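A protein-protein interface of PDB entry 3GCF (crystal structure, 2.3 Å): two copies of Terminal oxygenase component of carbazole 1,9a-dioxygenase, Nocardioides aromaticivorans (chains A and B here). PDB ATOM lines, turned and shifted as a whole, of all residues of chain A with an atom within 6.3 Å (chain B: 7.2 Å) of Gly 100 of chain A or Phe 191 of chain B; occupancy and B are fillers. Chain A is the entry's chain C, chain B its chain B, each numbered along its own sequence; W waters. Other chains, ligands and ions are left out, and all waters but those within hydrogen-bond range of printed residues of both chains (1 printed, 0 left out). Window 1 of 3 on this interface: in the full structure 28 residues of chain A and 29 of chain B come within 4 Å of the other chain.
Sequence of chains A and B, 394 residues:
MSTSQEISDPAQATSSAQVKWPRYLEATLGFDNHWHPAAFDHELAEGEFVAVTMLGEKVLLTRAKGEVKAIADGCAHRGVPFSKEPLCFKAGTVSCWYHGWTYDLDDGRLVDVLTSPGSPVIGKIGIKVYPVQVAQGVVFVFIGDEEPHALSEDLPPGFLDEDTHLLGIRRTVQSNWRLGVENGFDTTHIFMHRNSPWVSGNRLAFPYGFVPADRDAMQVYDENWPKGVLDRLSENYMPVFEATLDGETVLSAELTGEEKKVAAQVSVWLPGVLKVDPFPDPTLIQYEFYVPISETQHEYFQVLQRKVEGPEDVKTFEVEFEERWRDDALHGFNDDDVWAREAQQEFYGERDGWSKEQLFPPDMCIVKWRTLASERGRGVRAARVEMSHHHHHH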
ATOM      1  N   LEU A  87     -21.610   4.006 -22.735  1.00  0.00           N
ATOM      2  CA  LEU A  87     -22.534   3.593 -21.689  1.00  0.00           C
ATOM      3  C   LEU A  87     -22.160   4.148 -20.328  1.00  0.00           C
ATOM      4  O   LEU A  87     -20.983   4.256 -19.988  1.00  0.00           O
ATOM      5  CB  LEU A  87     -22.581   2.063 -21.599  1.00  0.00           C
ATOM      6  CG  LEU A  87     -23.073   1.285 -22.820  1.00  0.00           C
ATOM      7  CD1 LEU A  87     -22.814  -0.199 -22.615  1.00  0.00           C
ATOM      8  CD2 LEU A  87     -24.557   1.547 -23.035  1.00  0.00           C
ATOM      9  N   PHE A  89     -23.737   3.686 -16.320  1.00  0.00           N
ATOM     10  CA  PHE A  89     -24.748   3.133 -15.431  1.00  0.00           C
ATOM     11  C   PHE A  89     -24.685   3.774 -14.062  1.00  0.00           C
ATOM     12  O   PHE A  89     -25.523   3.512 -13.206  1.00  0.00           O
ATOM     13  CB  PHE A  89     -24.574   1.623 -15.333  1.00  0.00           C
ATOM     14  CG  PHE A  89     -24.819   0.915 -16.629  1.00  0.00           C
ATOM     15  CD1 PHE A  89     -26.110   0.799 -17.134  1.00  0.00           C
ATOM     16  CD2 PHE A  89     -23.761   0.402 -17.366  1.00  0.00           C
ATOM     17  CE1 PHE A  89     -26.342   0.177 -18.362  1.00  0.00           C
ATOM     18  CE2 PHE A  89     -23.982  -0.218 -18.592  1.00  0.00           C
ATOM     19  CZ  PHE A  89     -25.274  -0.331 -19.091  1.00  0.00           C
ATOM     20  N   VAL A  94     -17.763   5.125 -16.668  1.00  0.00           N
ATOM     21  CA  VAL A  94     -18.089   4.841 -18.047  1.00  0.00           C
ATOM     22  C   VAL A  94     -17.912   3.336 -18.162  1.00  0.00           C
ATOM     23  O   VAL A  94     -16.991   2.770 -17.566  1.00  0.00           O
ATOM     24  CB  VAL A  94     -17.162   5.586 -19.051  1.00  0.00           C
ATOM     25  CG1 VAL A  94     -15.719   5.119 -18.913  1.00  0.00           C
ATOM     26  CG2 VAL A  94     -17.675   5.356 -20.475  1.00  0.00           C
ATOM     27  N   SER A  95     -18.817   2.684 -18.885  1.00  0.00           N
ATOM     28  CA  SER A  95     -18.743   1.237 -19.057  1.00  0.00           C
ATOM     29  C   SER A  95     -18.573   0.885 -20.524  1.00  0.00           C
ATOM     30  O   SER A  95     -19.296   1.393 -21.377  1.00  0.00           O
ATOM     31  CB  SER A  95     -20.011   0.565 -18.516  1.00  0.00           C
ATOM     32  OG  SER A  95     -20.110   0.687 -17.105  1.00  0.00           O
ATOM     33  N   CYS A  96     -17.613   0.016 -20.814  1.00  0.00           N
ATOM     34  CA  CYS A  96     -17.370  -0.401 -22.185  1.00  0.00           C
ATOM     35  C   CYS A  96     -18.570  -1.219 -22.662  1.00  0.00           C
ATOM     36  O   CYS A  96     -19.118  -2.024 -21.913  1.00  0.00           O
ATOM     37  CB  CYS A  96     -16.098  -1.236 -22.260  1.00  0.00           C
ATOM     38  SG  CYS A  96     -15.618  -1.686 -23.935  1.00  0.00           S
ATOM     39  N   TRP A  97     -18.973  -1.005 -23.908  1.00  0.00           N
ATOM     40  CA  TRP A  97     -20.107  -1.705 -24.489  1.00  0.00           C
ATOM     41  C   TRP A  97     -19.814  -3.163 -24.839  1.00  0.00           C
ATOM     42  O   TRP A  97     -20.737  -3.942 -25.089  1.00  0.00           O
ATOM     43  CB  TRP A  97     -20.553  -0.998 -25.770  1.00  0.00           C
ATOM     44  CG  TRP A  97     -19.420  -0.787 -26.754  1.00  0.00           C
ATOM     45  CD1 TRP A  97     -18.626   0.324 -26.870  1.00  0.00           C
ATOM     46  CD2 TRP A  97     -18.919  -1.735 -27.709  1.00  0.00           C
ATOM     47  NE1 TRP A  97     -17.663   0.124 -27.837  1.00  0.00           N
ATOM     48  CE2 TRP A  97     -17.820  -1.129 -28.366  1.00  0.00           C
ATOM     49  CE3 TRP A  97     -19.290  -3.038 -28.071  1.00  0.00           C
ATOM     50  CZ2 TRP A  97     -17.086  -1.786 -29.367  1.00  0.00           C
ATOM     51  CZ3 TRP A  97     -18.558  -3.691 -29.064  1.00  0.00           C
ATOM     52  CH2 TRP A  97     -17.470  -3.063 -29.699  1.00  0.00           C
ATOM     53  N   TYR A  98     -18.539  -3.535 -24.856  1.00  0.00           N
ATOM     54  CA  TYR A  98     -18.169  -4.886 -25.262  1.00  0.00           C
ATOM     55  C   TYR A  98     -18.230  -5.958 -24.170  1.00  0.00           C
ATOM     56  O   TYR A  98     -19.015  -6.898 -24.289  1.00  0.00           O
ATOM     57  CB  TYR A  98     -16.785  -4.846 -25.925  1.00  0.00           C
ATOM     58  CG  TYR A  98     -16.546  -5.908 -26.979  1.00  0.00           C
ATOM     59  CD1 TYR A  98     -17.595  -6.681 -27.486  1.00  0.00           C
ATOM     60  CD2 TYR A  98     -15.256  -6.164 -27.453  1.00  0.00           C
ATOM     61  CE1 TYR A  98     -17.361  -7.688 -28.431  1.00  0.00           C
ATOM     62  CE2 TYR A  98     -15.012  -7.166 -28.390  1.00  0.00           C
ATOM     63  CZ  TYR A  98     -16.069  -7.927 -28.872  1.00  0.00           C
ATOM     64  OH  TYR A  98     -15.818  -8.940 -29.774  1.00  0.00           O
ATOM     65  N   HIS A  99     -17.412  -5.835 -23.121  1.00  0.00           N
ATOM     66  CA  HIS A  99     -17.433  -6.820 -22.034  1.00  0.00           C
ATOM     67  C   HIS A  99     -17.763  -6.170 -20.693  1.00  0.00           C
ATOM     68  O   HIS A  99     -17.570  -6.772 -19.631  1.00  0.00           O
ATOM     69  CB  HIS A  99     -16.093  -7.556 -21.913  1.00  0.00           C
ATOM     70  CG  HIS A  99     -15.592  -8.127 -23.203  1.00  0.00           C
ATOM     71  ND1 HIS A  99     -14.830  -7.399 -24.091  1.00  0.00           N
ATOM     72  CD2 HIS A  99     -15.757  -9.350 -23.760  1.00  0.00           C
ATOM     73  CE1 HIS A  99     -14.547  -8.151 -25.141  1.00  0.00           C
ATOM     74  NE2 HIS A  99     -15.098  -9.339 -24.965  1.00  0.00           N
ATOM     75  N   GLY A 100     -18.242  -4.930 -20.743  1.00  0.00           N
ATOM     76  CA  GLY A 100     -18.624  -4.243 -19.526  1.00  0.00           C
ATOM     77  C   GLY A 100     -17.554  -3.718 -18.584  1.00  0.00           C
ATOM     78  O   GLY A 100     -17.861  -3.421 -17.432  1.00  0.00           O
ATOM     79  N   TRP A 101     -16.308  -3.612 -19.034  1.00  0.00           N
ATOM     80  CA  TRP A 101     -15.278  -3.062 -18.155  1.00  0.00           C
ATOM     81  C   TRP A 101     -15.730  -1.638 -17.826  1.00  0.00           C
ATOM     82  O   TRP A 101     -16.090  -0.869 -18.720  1.00  0.00           O
ATOM     83  CB  TRP A 101     -13.918  -3.062 -18.852  1.00  0.00           C
ATOM     84  CG  TRP A 101     -13.259  -4.419 -18.865  1.00  0.00           C
ATOM     85  CD1 TRP A 101     -13.880  -5.642 -18.895  1.00  0.00           C
ATOM     86  CD2 TRP A 101     -11.851  -4.686 -18.895  1.00  0.00           C
ATOM     87  NE1 TRP A 101     -12.945  -6.649 -18.942  1.00  0.00           N
ATOM     88  CE2 TRP A 101     -11.692  -6.091 -18.945  1.00  0.00           C
ATOM     89  CE3 TRP A 101     -10.706  -3.873 -18.886  1.00  0.00           C
ATOM     90  CZ2 TRP A 101     -10.433  -6.701 -18.988  1.00  0.00           C
ATOM     91  CZ3 TRP A 101      -9.458  -4.479 -18.929  1.00  0.00           C
ATOM     92  CH2 TRP A 101      -9.331  -5.884 -18.978  1.00  0.00           C
ATOM     93  N   THR A 102     -15.720  -1.297 -16.542  1.00  0.00           N
ATOM     94  CA  THR A 102     -16.184   0.008 -16.089  1.00  0.00           C
ATOM     95  C   THR A 102     -15.072   0.812 -15.434  1.00  0.00           C
ATOM     96  O   THR A 102     -14.346   0.313 -14.574  1.00  0.00           O
ATOM     97  CB  THR A 102     -17.360  -0.184 -15.112  1.00  0.00           C
ATOM     98  OG1 THR A 102     -18.380  -0.949 -15.768  1.00  0.00           O
ATOM     99  CG2 THR A 102     -17.940   1.153 -14.671  1.00  0.00           C
ATOM    100  N   LEU A 110      -9.891   0.871 -13.486  1.00  0.00           N
ATOM    101  CA  LEU A 110     -10.934  -0.122 -13.716  1.00  0.00           C
ATOM    102  C   LEU A 110     -11.521  -0.421 -12.329  1.00  0.00           C
ATOM    103  O   LEU A 110     -10.815  -0.918 -11.453  1.00  0.00           O
ATOM    104  CB  LEU A 110     -10.323  -1.394 -14.306  1.00  0.00           C
ATOM    105  CG  LEU A 110     -11.287  -2.554 -14.571  1.00  0.00           C
ATOM    106  CD1 LEU A 110     -12.288  -2.139 -15.639  1.00  0.00           C
ATOM    107  CD2 LEU A 110     -10.511  -3.784 -15.013  1.00  0.00           C
ATOM    108  N   ASP A 112     -14.704  -2.011 -12.004  1.00  0.00           N
ATOM    109  CA  ASP A 112     -15.667  -3.093 -12.088  1.00  0.00           C
ATOM    110  C   ASP A 112     -15.728  -3.728 -13.464  1.00  0.00           C
ATOM    111  O   ASP A 112     -15.204  -3.189 -14.439  1.00  0.00           O
ATOM    112  CB  ASP A 112     -17.063  -2.591 -11.708  1.00  0.00           C
ATOM    113  CG  ASP A 112     -17.828  -3.591 -10.860  1.00  0.00           C
ATOM    114  OD1 ASP A 112     -17.775  -4.803 -11.184  1.00  0.00           O
ATOM    115  OD2 ASP A 112     -18.477  -3.167  -9.874  1.00  0.00           O
ATOM    116  N   VAL A 113     -16.364  -4.891 -13.522  1.00  0.00           N
ATOM    117  CA  VAL A 113     -16.556  -5.622 -14.765  1.00  0.00           C
ATOM    118  C   VAL A 113     -17.948  -6.224 -14.679  1.00  0.00           C
ATOM    119  O   VAL A 113     -18.180  -7.216 -13.982  1.00  0.00           O
ATOM    120  CB  VAL A 113     -15.501  -6.727 -14.945  1.00  0.00           C
ATOM    121  CG1 VAL A 113     -15.725  -7.453 -16.275  1.00  0.00           C
ATOM    122  CG2 VAL A 113     -14.108  -6.111 -14.918  1.00  0.00           C
ATOM    123  N   LEU A 114     -18.877  -5.591 -15.386  1.00  0.00           N
ATOM    124  CA  LEU A 114     -20.274  -6.001 -15.397  1.00  0.00           C
ATOM    125  C   LEU A 114     -20.524  -7.461 -15.757  1.00  0.00           C
ATOM    126  O   LEU A 114     -21.513  -8.045 -15.313  1.00  0.00           O
ATOM    127  CB  LEU A 114     -21.056  -5.100 -16.350  1.00  0.00           C
ATOM    128  CG  LEU A 114     -20.953  -3.608 -16.017  1.00  0.00           C
ATOM    129  CD1 LEU A 114     -21.701  -2.803 -17.065  1.00  0.00           C
ATOM    130  CD2 LEU A 114     -21.517  -3.349 -14.620  1.00  0.00           C
ATOM    131  N   THR A 115     -19.632  -8.048 -16.552  1.00  0.00           N
ATOM    132  CA  THR A 115     -19.789  -9.435 -16.977  1.00  0.00           C
ATOM    133  C   THR A 115     -19.035 -10.415 -16.083  1.00  0.00           C
ATOM    134  O   THR A 115     -19.087 -11.627 -16.296  1.00  0.00           O
ATOM    135  CB  THR A 115     -19.276  -9.639 -18.416  1.00  0.00           C
ATOM    136  OG1 THR A 115     -17.898  -9.249 -18.490  1.00  0.00           O
ATOM    137  CG2 THR A 115     -20.098  -8.824 -19.400  1.00  0.00           C
ATOM    138  N   THR B 187     -16.704 -15.730 -24.320  1.00  0.00           N
ATOM    139  CA  THR B 187     -17.827 -15.976 -23.425  1.00  0.00           C
ATOM    140  C   THR B 187     -18.420 -14.805 -22.634  1.00  0.00           C
ATOM    141  O   THR B 187     -19.446 -14.971 -21.972  1.00  0.00           O
ATOM    142  CB  THR B 187     -17.500 -17.138 -22.440  1.00  0.00           C
ATOM    143  OG1 THR B 187     -16.538 -16.707 -21.473  1.00  0.00           O
ATOM    144  CG2 THR B 187     -16.922 -18.328 -23.203  1.00  0.00           C
ATOM    145  N   THR B 188     -17.803 -13.629 -22.694  1.00  0.00           N
ATOM    146  CA  THR B 188     -18.357 -12.487 -21.973  1.00  0.00           C
ATOM    147  C   THR B 188     -18.760 -11.321 -22.882  1.00  0.00           C
ATOM    148  O   THR B 188     -19.338 -10.340 -22.417  1.00  0.00           O
ATOM    149  CB  THR B 188     -17.396 -11.975 -20.865  1.00  0.00           C
ATOM    150  OG1 THR B 188     -16.156 -11.551 -21.442  1.00  0.00           O
ATOM    151  CG2 THR B 188     -17.140 -13.077 -19.848  1.00  0.00           C
ATOM    152  N   HIS B 189     -18.477 -11.428 -24.176  1.00  0.00           N
ATOM    153  CA  HIS B 189     -18.847 -10.361 -25.099  1.00  0.00           C
ATOM    154  C   HIS B 189     -20.365 -10.350 -25.311  1.00  0.00           C
ATOM    155  O   HIS B 189     -20.915  -9.376 -25.828  1.00  0.00           O
ATOM    156  CB  HIS B 189     -18.173 -10.554 -26.466  1.00  0.00           C
ATOM    157  CG  HIS B 189     -18.999 -11.347 -27.436  1.00  0.00           C
ATOM    158  ND1 HIS B 189     -19.101 -12.721 -27.383  1.00  0.00           N
ATOM    159  CD2 HIS B 189     -19.802 -10.950 -28.453  1.00  0.00           C
ATOM    160  CE1 HIS B 189     -19.932 -13.136 -28.324  1.00  0.00           C
ATOM    161  NE2 HIS B 189     -20.371 -12.081 -28.987  1.00  0.00           N
ATOM    162  N   ILE B 190     -21.037 -11.432 -24.917  1.00  0.00           N
ATOM    163  CA  ILE B 190     -22.479 -11.537 -25.123  1.00  0.00           C
ATOM    164  C   ILE B 190     -23.260 -10.437 -24.430  1.00  0.00           C
ATOM    165  O   ILE B 190     -24.454 -10.240 -24.685  1.00  0.00           O
ATOM    166  CB  ILE B 190     -23.021 -12.931 -24.705  1.00  0.00           C
ATOM    167  CG1 ILE B 190     -22.799 -13.177 -23.214  1.00  0.00           C
ATOM    168  CG2 ILE B 190     -22.337 -14.016 -25.547  1.00  0.00           C
ATOM    169  CD1 ILE B 190     -23.304 -14.538 -22.758  1.00  0.00           C
ATOM    170  N   PHE B 191     -22.566  -9.711 -23.563  1.00  0.00           N
ATOM    171  CA  PHE B 191     -23.138  -8.579 -22.850  1.00  0.00           C
ATOM    172  C   PHE B 191     -23.730  -7.619 -23.887  1.00  0.00           C
ATOM    173  O   PHE B 191     -24.826  -7.083 -23.700  1.00  0.00           O
ATOM    174  CB  PHE B 191     -22.021  -7.877 -22.067  1.00  0.00           C
ATOM    175  CG  PHE B 191     -22.387  -6.518 -21.543  1.00  0.00           C
ATOM    176  CD1 PHE B 191     -23.363  -6.368 -20.563  1.00  0.00           C
ATOM    177  CD2 PHE B 191     -21.722  -5.383 -22.004  1.00  0.00           C
ATOM    178  CE1 PHE B 191     -23.672  -5.107 -20.046  1.00  0.00           C
ATOM    179  CE2 PHE B 191     -22.024  -4.112 -21.492  1.00  0.00           C
ATOM    180  CZ  PHE B 191     -22.998  -3.975 -20.514  1.00  0.00           C
ATOM    181  N   MET B 192     -23.007  -7.426 -24.991  1.00  0.00           N
ATOM    182  CA  MET B 192     -23.440  -6.504 -26.042  1.00  0.00           C
ATOM    183  C   MET B 192     -24.686  -6.946 -26.801  1.00  0.00           C
ATOM    184  O   MET B 192     -25.269  -6.151 -27.537  1.00  0.00           O
ATOM    185  CB  MET B 192     -22.309  -6.264 -27.049  1.00  0.00           C
ATOM    186  CG  MET B 192     -22.174  -7.351 -28.106  1.00  0.00           C
ATOM    187  SD  MET B 192     -20.936  -7.001 -29.376  1.00  0.00           S
ATOM    188  CE  MET B 192     -21.725  -5.689 -30.258  1.00  0.00           C
ATOM    189  N   HIS B 193     -25.096  -8.200 -26.632  1.00  0.00           N
ATOM    190  CA  HIS B 193     -26.283  -8.711 -27.324  1.00  0.00           C
ATOM    191  C   HIS B 193     -27.544  -8.660 -26.458  1.00  0.00           C
ATOM    192  O   HIS B 193     -28.630  -9.013 -26.920  1.00  0.00           O
ATOM    193  CB  HIS B 193     -26.082 -10.174 -27.743  1.00  0.00           C
ATOM    194  CG  HIS B 193     -24.970 -10.392 -28.720  1.00  0.00           C
ATOM    195  ND1 HIS B 193     -24.929  -9.775 -29.952  1.00  0.00           N
ATOM    196  CD2 HIS B 193     -23.892 -11.212 -28.673  1.00  0.00           C
ATOM    197  CE1 HIS B 193     -23.876 -10.209 -30.623  1.00  0.00           C
ATOM    198  NE2 HIS B 193     -23.230 -11.082 -29.869  1.00  0.00           N
ATOM    199  N   ARG B 194     -27.398  -8.230 -25.208  1.00  0.00           N
ATOM    200  CA  ARG B 194     -28.515  -8.200 -24.265  1.00  0.00           C
ATOM    201  C   ARG B 194     -29.803  -7.557 -24.767  1.00  0.00           C
ATOM    202  O   ARG B 194     -30.898  -7.927 -24.329  1.00  0.00           O
ATOM    203  CB  ARG B 194     -28.081  -7.521 -22.958  1.00  0.00           C
ATOM    204  CG  ARG B 194     -27.802  -6.036 -23.092  1.00  0.00           C
ATOM    205  CD  ARG B 194     -27.230  -5.450 -21.809  1.00  0.00           C
ATOM    206  NE  ARG B 194     -27.056  -4.008 -21.926  1.00  0.00           N
ATOM    207  CZ  ARG B 194     -26.154  -3.420 -22.702  1.00  0.00           C
ATOM    208  NH1 ARG B 194     -25.324  -4.152 -23.430  1.00  0.00           N
ATOM    209  NH2 ARG B 194     -26.104  -2.097 -22.771  1.00  0.00           N
ATOM    210  N   ASN B 195     -29.689  -6.601 -25.681  1.00  0.00           N
ATOM    211  CA  ASN B 195     -30.881  -5.927 -26.189  1.00  0.00           C
ATOM    212  C   ASN B 195     -31.358  -6.383 -27.561  1.00  0.00           C
ATOM    213  O   ASN B 195     -32.270  -5.792 -28.124  1.00  0.00           O
ATOM    214  CB  ASN B 195     -30.674  -4.410 -26.188  1.00  0.00           C
ATOM    215  CG  ASN B 195     -30.609  -3.836 -24.782  1.00  0.00           C
ATOM    216  OD1 ASN B 195     -31.425  -4.184 -23.924  1.00  0.00           O
ATOM    217  ND2 ASN B 195     -29.645  -2.949 -24.540  1.00  0.00           N
ATOM    218  N   PHE B 206     -31.023 -15.532 -21.382  1.00  0.00           N
ATOM    219  CA  PHE B 206     -29.697 -15.189 -21.874  1.00  0.00           C
ATOM    220  C   PHE B 206     -28.914 -14.340 -20.889  1.00  0.00           C
ATOM    221  O   PHE B 206     -29.314 -13.226 -20.568  1.00  0.00           O
ATOM    222  CB  PHE B 206     -29.840 -14.457 -23.209  1.00  0.00           C
ATOM    223  CG  PHE B 206     -28.625 -14.534 -24.075  1.00  0.00           C
ATOM    224  CD1 PHE B 206     -28.211 -15.753 -24.603  1.00  0.00           C
ATOM    225  CD2 PHE B 206     -27.895 -13.390 -24.371  1.00  0.00           C
ATOM    226  CE1 PHE B 206     -27.086 -15.829 -25.421  1.00  0.00           C
ATOM    227  CE2 PHE B 206     -26.768 -13.458 -25.187  1.00  0.00           C
ATOM    228  CZ  PHE B 206     -26.364 -14.678 -25.712  1.00  0.00           C
ATOM    229  N   PRO B 207     -27.770 -14.854 -20.408  1.00  0.00           N
ATOM    230  CA  PRO B 207     -26.936 -14.131 -19.449  1.00  0.00           C
ATOM    231  C   PRO B 207     -26.084 -13.040 -20.090  1.00  0.00           C
ATOM    232  O   PRO B 207     -26.004 -12.946 -21.314  1.00  0.00           O
ATOM    233  CB  PRO B 207     -26.098 -15.244 -18.830  1.00  0.00           C
ATOM    234  CG  PRO B 207     -25.854 -16.141 -19.995  1.00  0.00           C
ATOM    235  CD  PRO B 207     -27.218 -16.197 -20.674  1.00  0.00           C
ATOM    236  N   TYR B 208     -25.461 -12.210 -19.254  1.00  0.00           N
ATOM    237  CA  TYR B 208     -24.599 -11.142 -19.736  1.00  0.00           C
ATOM    238  C   TYR B 208     -23.200 -11.688 -19.992  1.00  0.00           C
ATOM    239  O   TYR B 208     -22.366 -11.033 -20.621  1.00  0.00           O
ATOM    240  CB  TYR B 208     -24.529  -9.999 -18.715  1.00  0.00           C
ATOM    241  CG  TYR B 208     -25.846  -9.285 -18.508  1.00  0.00           C
ATOM    242  CD1 TYR B 208     -26.651  -8.950 -19.594  1.00  0.00           C
ATOM    243  CD2 TYR B 208     -26.285  -8.937 -17.231  1.00  0.00           C
ATOM    244  CE1 TYR B 208     -27.859  -8.289 -19.422  1.00  0.00           C
ATOM    245  CE2 TYR B 208     -27.504  -8.270 -17.049  1.00  0.00           C
ATOM    246  CZ  TYR B 208     -28.282  -7.954 -18.154  1.00  0.00           C
ATOM    247  OH  TYR B 208     -29.497  -7.324 -18.003  1.00  0.00           O
ATOM    248  N   GLY B 209     -22.950 -12.895 -19.497  1.00  0.00           N
ATOM    249  CA  GLY B 209     -21.652 -13.515 -19.686  1.00  0.00           C
ATOM    250  C   GLY B 209     -21.509 -14.838 -18.960  1.00  0.00           C
ATOM    251  O   GLY B 209     -22.334 -15.180 -18.113  1.00  0.00           O
ATOM    252  N   ALA B 243     -26.128  -7.462 -13.604  1.00  0.00           N
ATOM    253  CA  ALA B 243     -24.952  -6.605 -13.689  1.00  0.00           C
ATOM    254  C   ALA B 243     -24.990  -5.659 -12.497  1.00  0.00           C
ATOM    255  O   ALA B 243     -26.005  -5.013 -12.239  1.00  0.00           O
ATOM    256  CB  ALA B 243     -24.960  -5.810 -14.985  1.00  0.00           C
ATOM    257  N   LEU B 251     -28.480  -3.618 -13.989  1.00  0.00           N
ATOM    258  CA  LEU B 251     -29.019  -4.330 -15.137  1.00  0.00           C
ATOM    259  C   LEU B 251     -29.319  -5.767 -14.734  1.00  0.00           C
ATOM    260  O   LEU B 251     -28.573  -6.365 -13.969  1.00  0.00           O
ATOM    261  CB  LEU B 251     -27.975  -4.320 -16.258  1.00  0.00           C
ATOM    262  CG  LEU B 251     -28.280  -3.827 -17.675  1.00  0.00           C
ATOM    263  CD1 LEU B 251     -29.059  -2.520 -17.670  1.00  0.00           C
ATOM    264  CD2 LEU B 251     -26.945  -3.648 -18.393  1.00  0.00           C
ATOM    265  N   PHE B 360      -8.427 -10.829 -19.358  1.00  0.00           N
ATOM    266  CA  PHE B 360      -8.858 -11.221 -18.028  1.00  0.00           C
ATOM    267  C   PHE B 360      -9.281 -12.694 -18.075  1.00  0.00           C
ATOM    268  O   PHE B 360      -9.473 -13.249 -19.155  1.00  0.00           O
ATOM    269  CB  PHE B 360      -9.924 -10.242 -17.464  1.00  0.00           C
ATOM    270  CG  PHE B 360     -11.306 -10.357 -18.062  1.00  0.00           C
ATOM    271  CD1 PHE B 360     -11.509 -10.343 -19.435  1.00  0.00           C
ATOM    272  CD2 PHE B 360     -12.423 -10.378 -17.221  1.00  0.00           C
ATOM    273  CE1 PHE B 360     -12.807 -10.343 -19.966  1.00  0.00           C
ATOM    274  CE2 PHE B 360     -13.724 -10.378 -17.738  1.00  0.00           C
ATOM    275  CZ  PHE B 360     -13.913 -10.359 -19.111  1.00  0.00           C
HETATM  276  O   HOH W   1     -23.260  -3.128 -25.003  1.00  0.00           O
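The guanidinium group of Arg 194 of chain B is in hydrogen-bond range of the backbone carbonyl oxygen of Phe 191 of chain B (3.0 Å). The backbone NH (N) of Ala 243 of chain B sits at hydrogen-bond distance from the backbone carbonyl oxygen (O) of Leu 251 of chain B, 2.7 Å away. The side-chain sulfur of Cys 96 of chain A lies close to the backbone NH of Tyr 98 of chain A (3.6 Å). The backbone carbonyl oxygen (O) of Trp 101 of chain A lies within hydrogen-bond range of the backbone NH (N) of Cys 96 of chain A (2.7 Å). O of His 99 of chain A is in hydrogen-bond range of OG1 of Thr 115 of chain A (2.7 Å). The side-chain hydroxyl (OG1) of Thr 102 of chain A sits at hydrogen-bond distance from the backbone carbonyl oxygen (O) of Gly 100 of chain A (3.0 Å).
Water W1 lies within hydrogen-bond range of O of Trp 97 of chain A (2.7 Å) and NH1 of Arg 194 of chain B (2.8 Å).
Of the 16 printed residues of chain B, 8 touch a printed residue of chain A. Hydrophobic or aromatic side chains of chain B that line the printed part of chain A: His 189, Phe 191, Met 192, Leu 251 and Phe 360. Along chain B the printed residues that touch a printed residue of chain A span positions 188 to 360. Printed residues of chain A that touch a printed residue of chain B: Leu 87, Phe 89, Cys 96, Trp 97, Tyr 98, His 99, Gly 100, Trp 101, Val 113, Leu 114 and Thr 115. Hydrophobic or aromatic side chains of chain A that line the printed part of chain B: Leu 87, Phe 89, Trp 97, Tyr 98, His 99, Trp 101, Val 113 and Leu 114. Along chain A the printed residues that touch a printed residue of chain B span positions 87 to 115. Among the printed residues, 18 pairs touch across the chains. Among the printed residues, no Asp or Glu carboxylate lies within 4 Å of a Lys or Arg side-chain nitrogen of the other chain.
O of Tyr 98 of chain A lies close to O of His 189 of chain B (3.5 Å).
Printed residues of chain B within 4 Å of Tyr 98 of chain A: Thr 188, His 189, Phe 191 and Met 192. Of chain B, only Phe 191 comes within 4 Å of Gly 100 of chain A. Printed residues of chain B within 4 Å of Trp 101 of chain A: Phe 360 (3.8 Å). Phe 191 of chain B touches six residues of chain A. The nearest residue of chain B that does not touch Gly 100 of chain A is Thr 188 of chain B (5.8 Å). The nearest printed residue of chain B that does not touch Val 113 of chain A is Thr 188 of chain B (6.6 Å).
No position is printed for both chains. Of the 18 pairs that touch across the chains among the printed residues, none has its exchanged pair printed and touching as well.
Arg 194 of chain B touches Leu 87 of chain A (NH2 to CD1, 3.8 Å). Trp 97 of chain A touches Phe 191 of chain B. O of Trp 97 of chain A touches CB of Met 192 of chain B, 3.4 Å away. Tyr 98 of chain A touches Thr 188 of chain B (O to O, 3.9 Å). O of Tyr 98 of chain A touches CD2 of Phe 191 of chain B (3.9 Å). Thr 188 of chain B touches His 99 of chain A (OG1 to CD2, 3.2 Å). Gly 100 of chain A touches Phe 191 of chain B (N to CD2, 3.7 Å). CD1 of Leu 114 of chain A touches CZ of Phe 191 of chain B, 3.9 Å away. Thr 115 of chain A touches Phe 191 of chain B (CG2 to CB, 3.4 Å). O of Tyr 208 of chain B touches CG2 of Thr 115 of chain A (3.4 Å).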
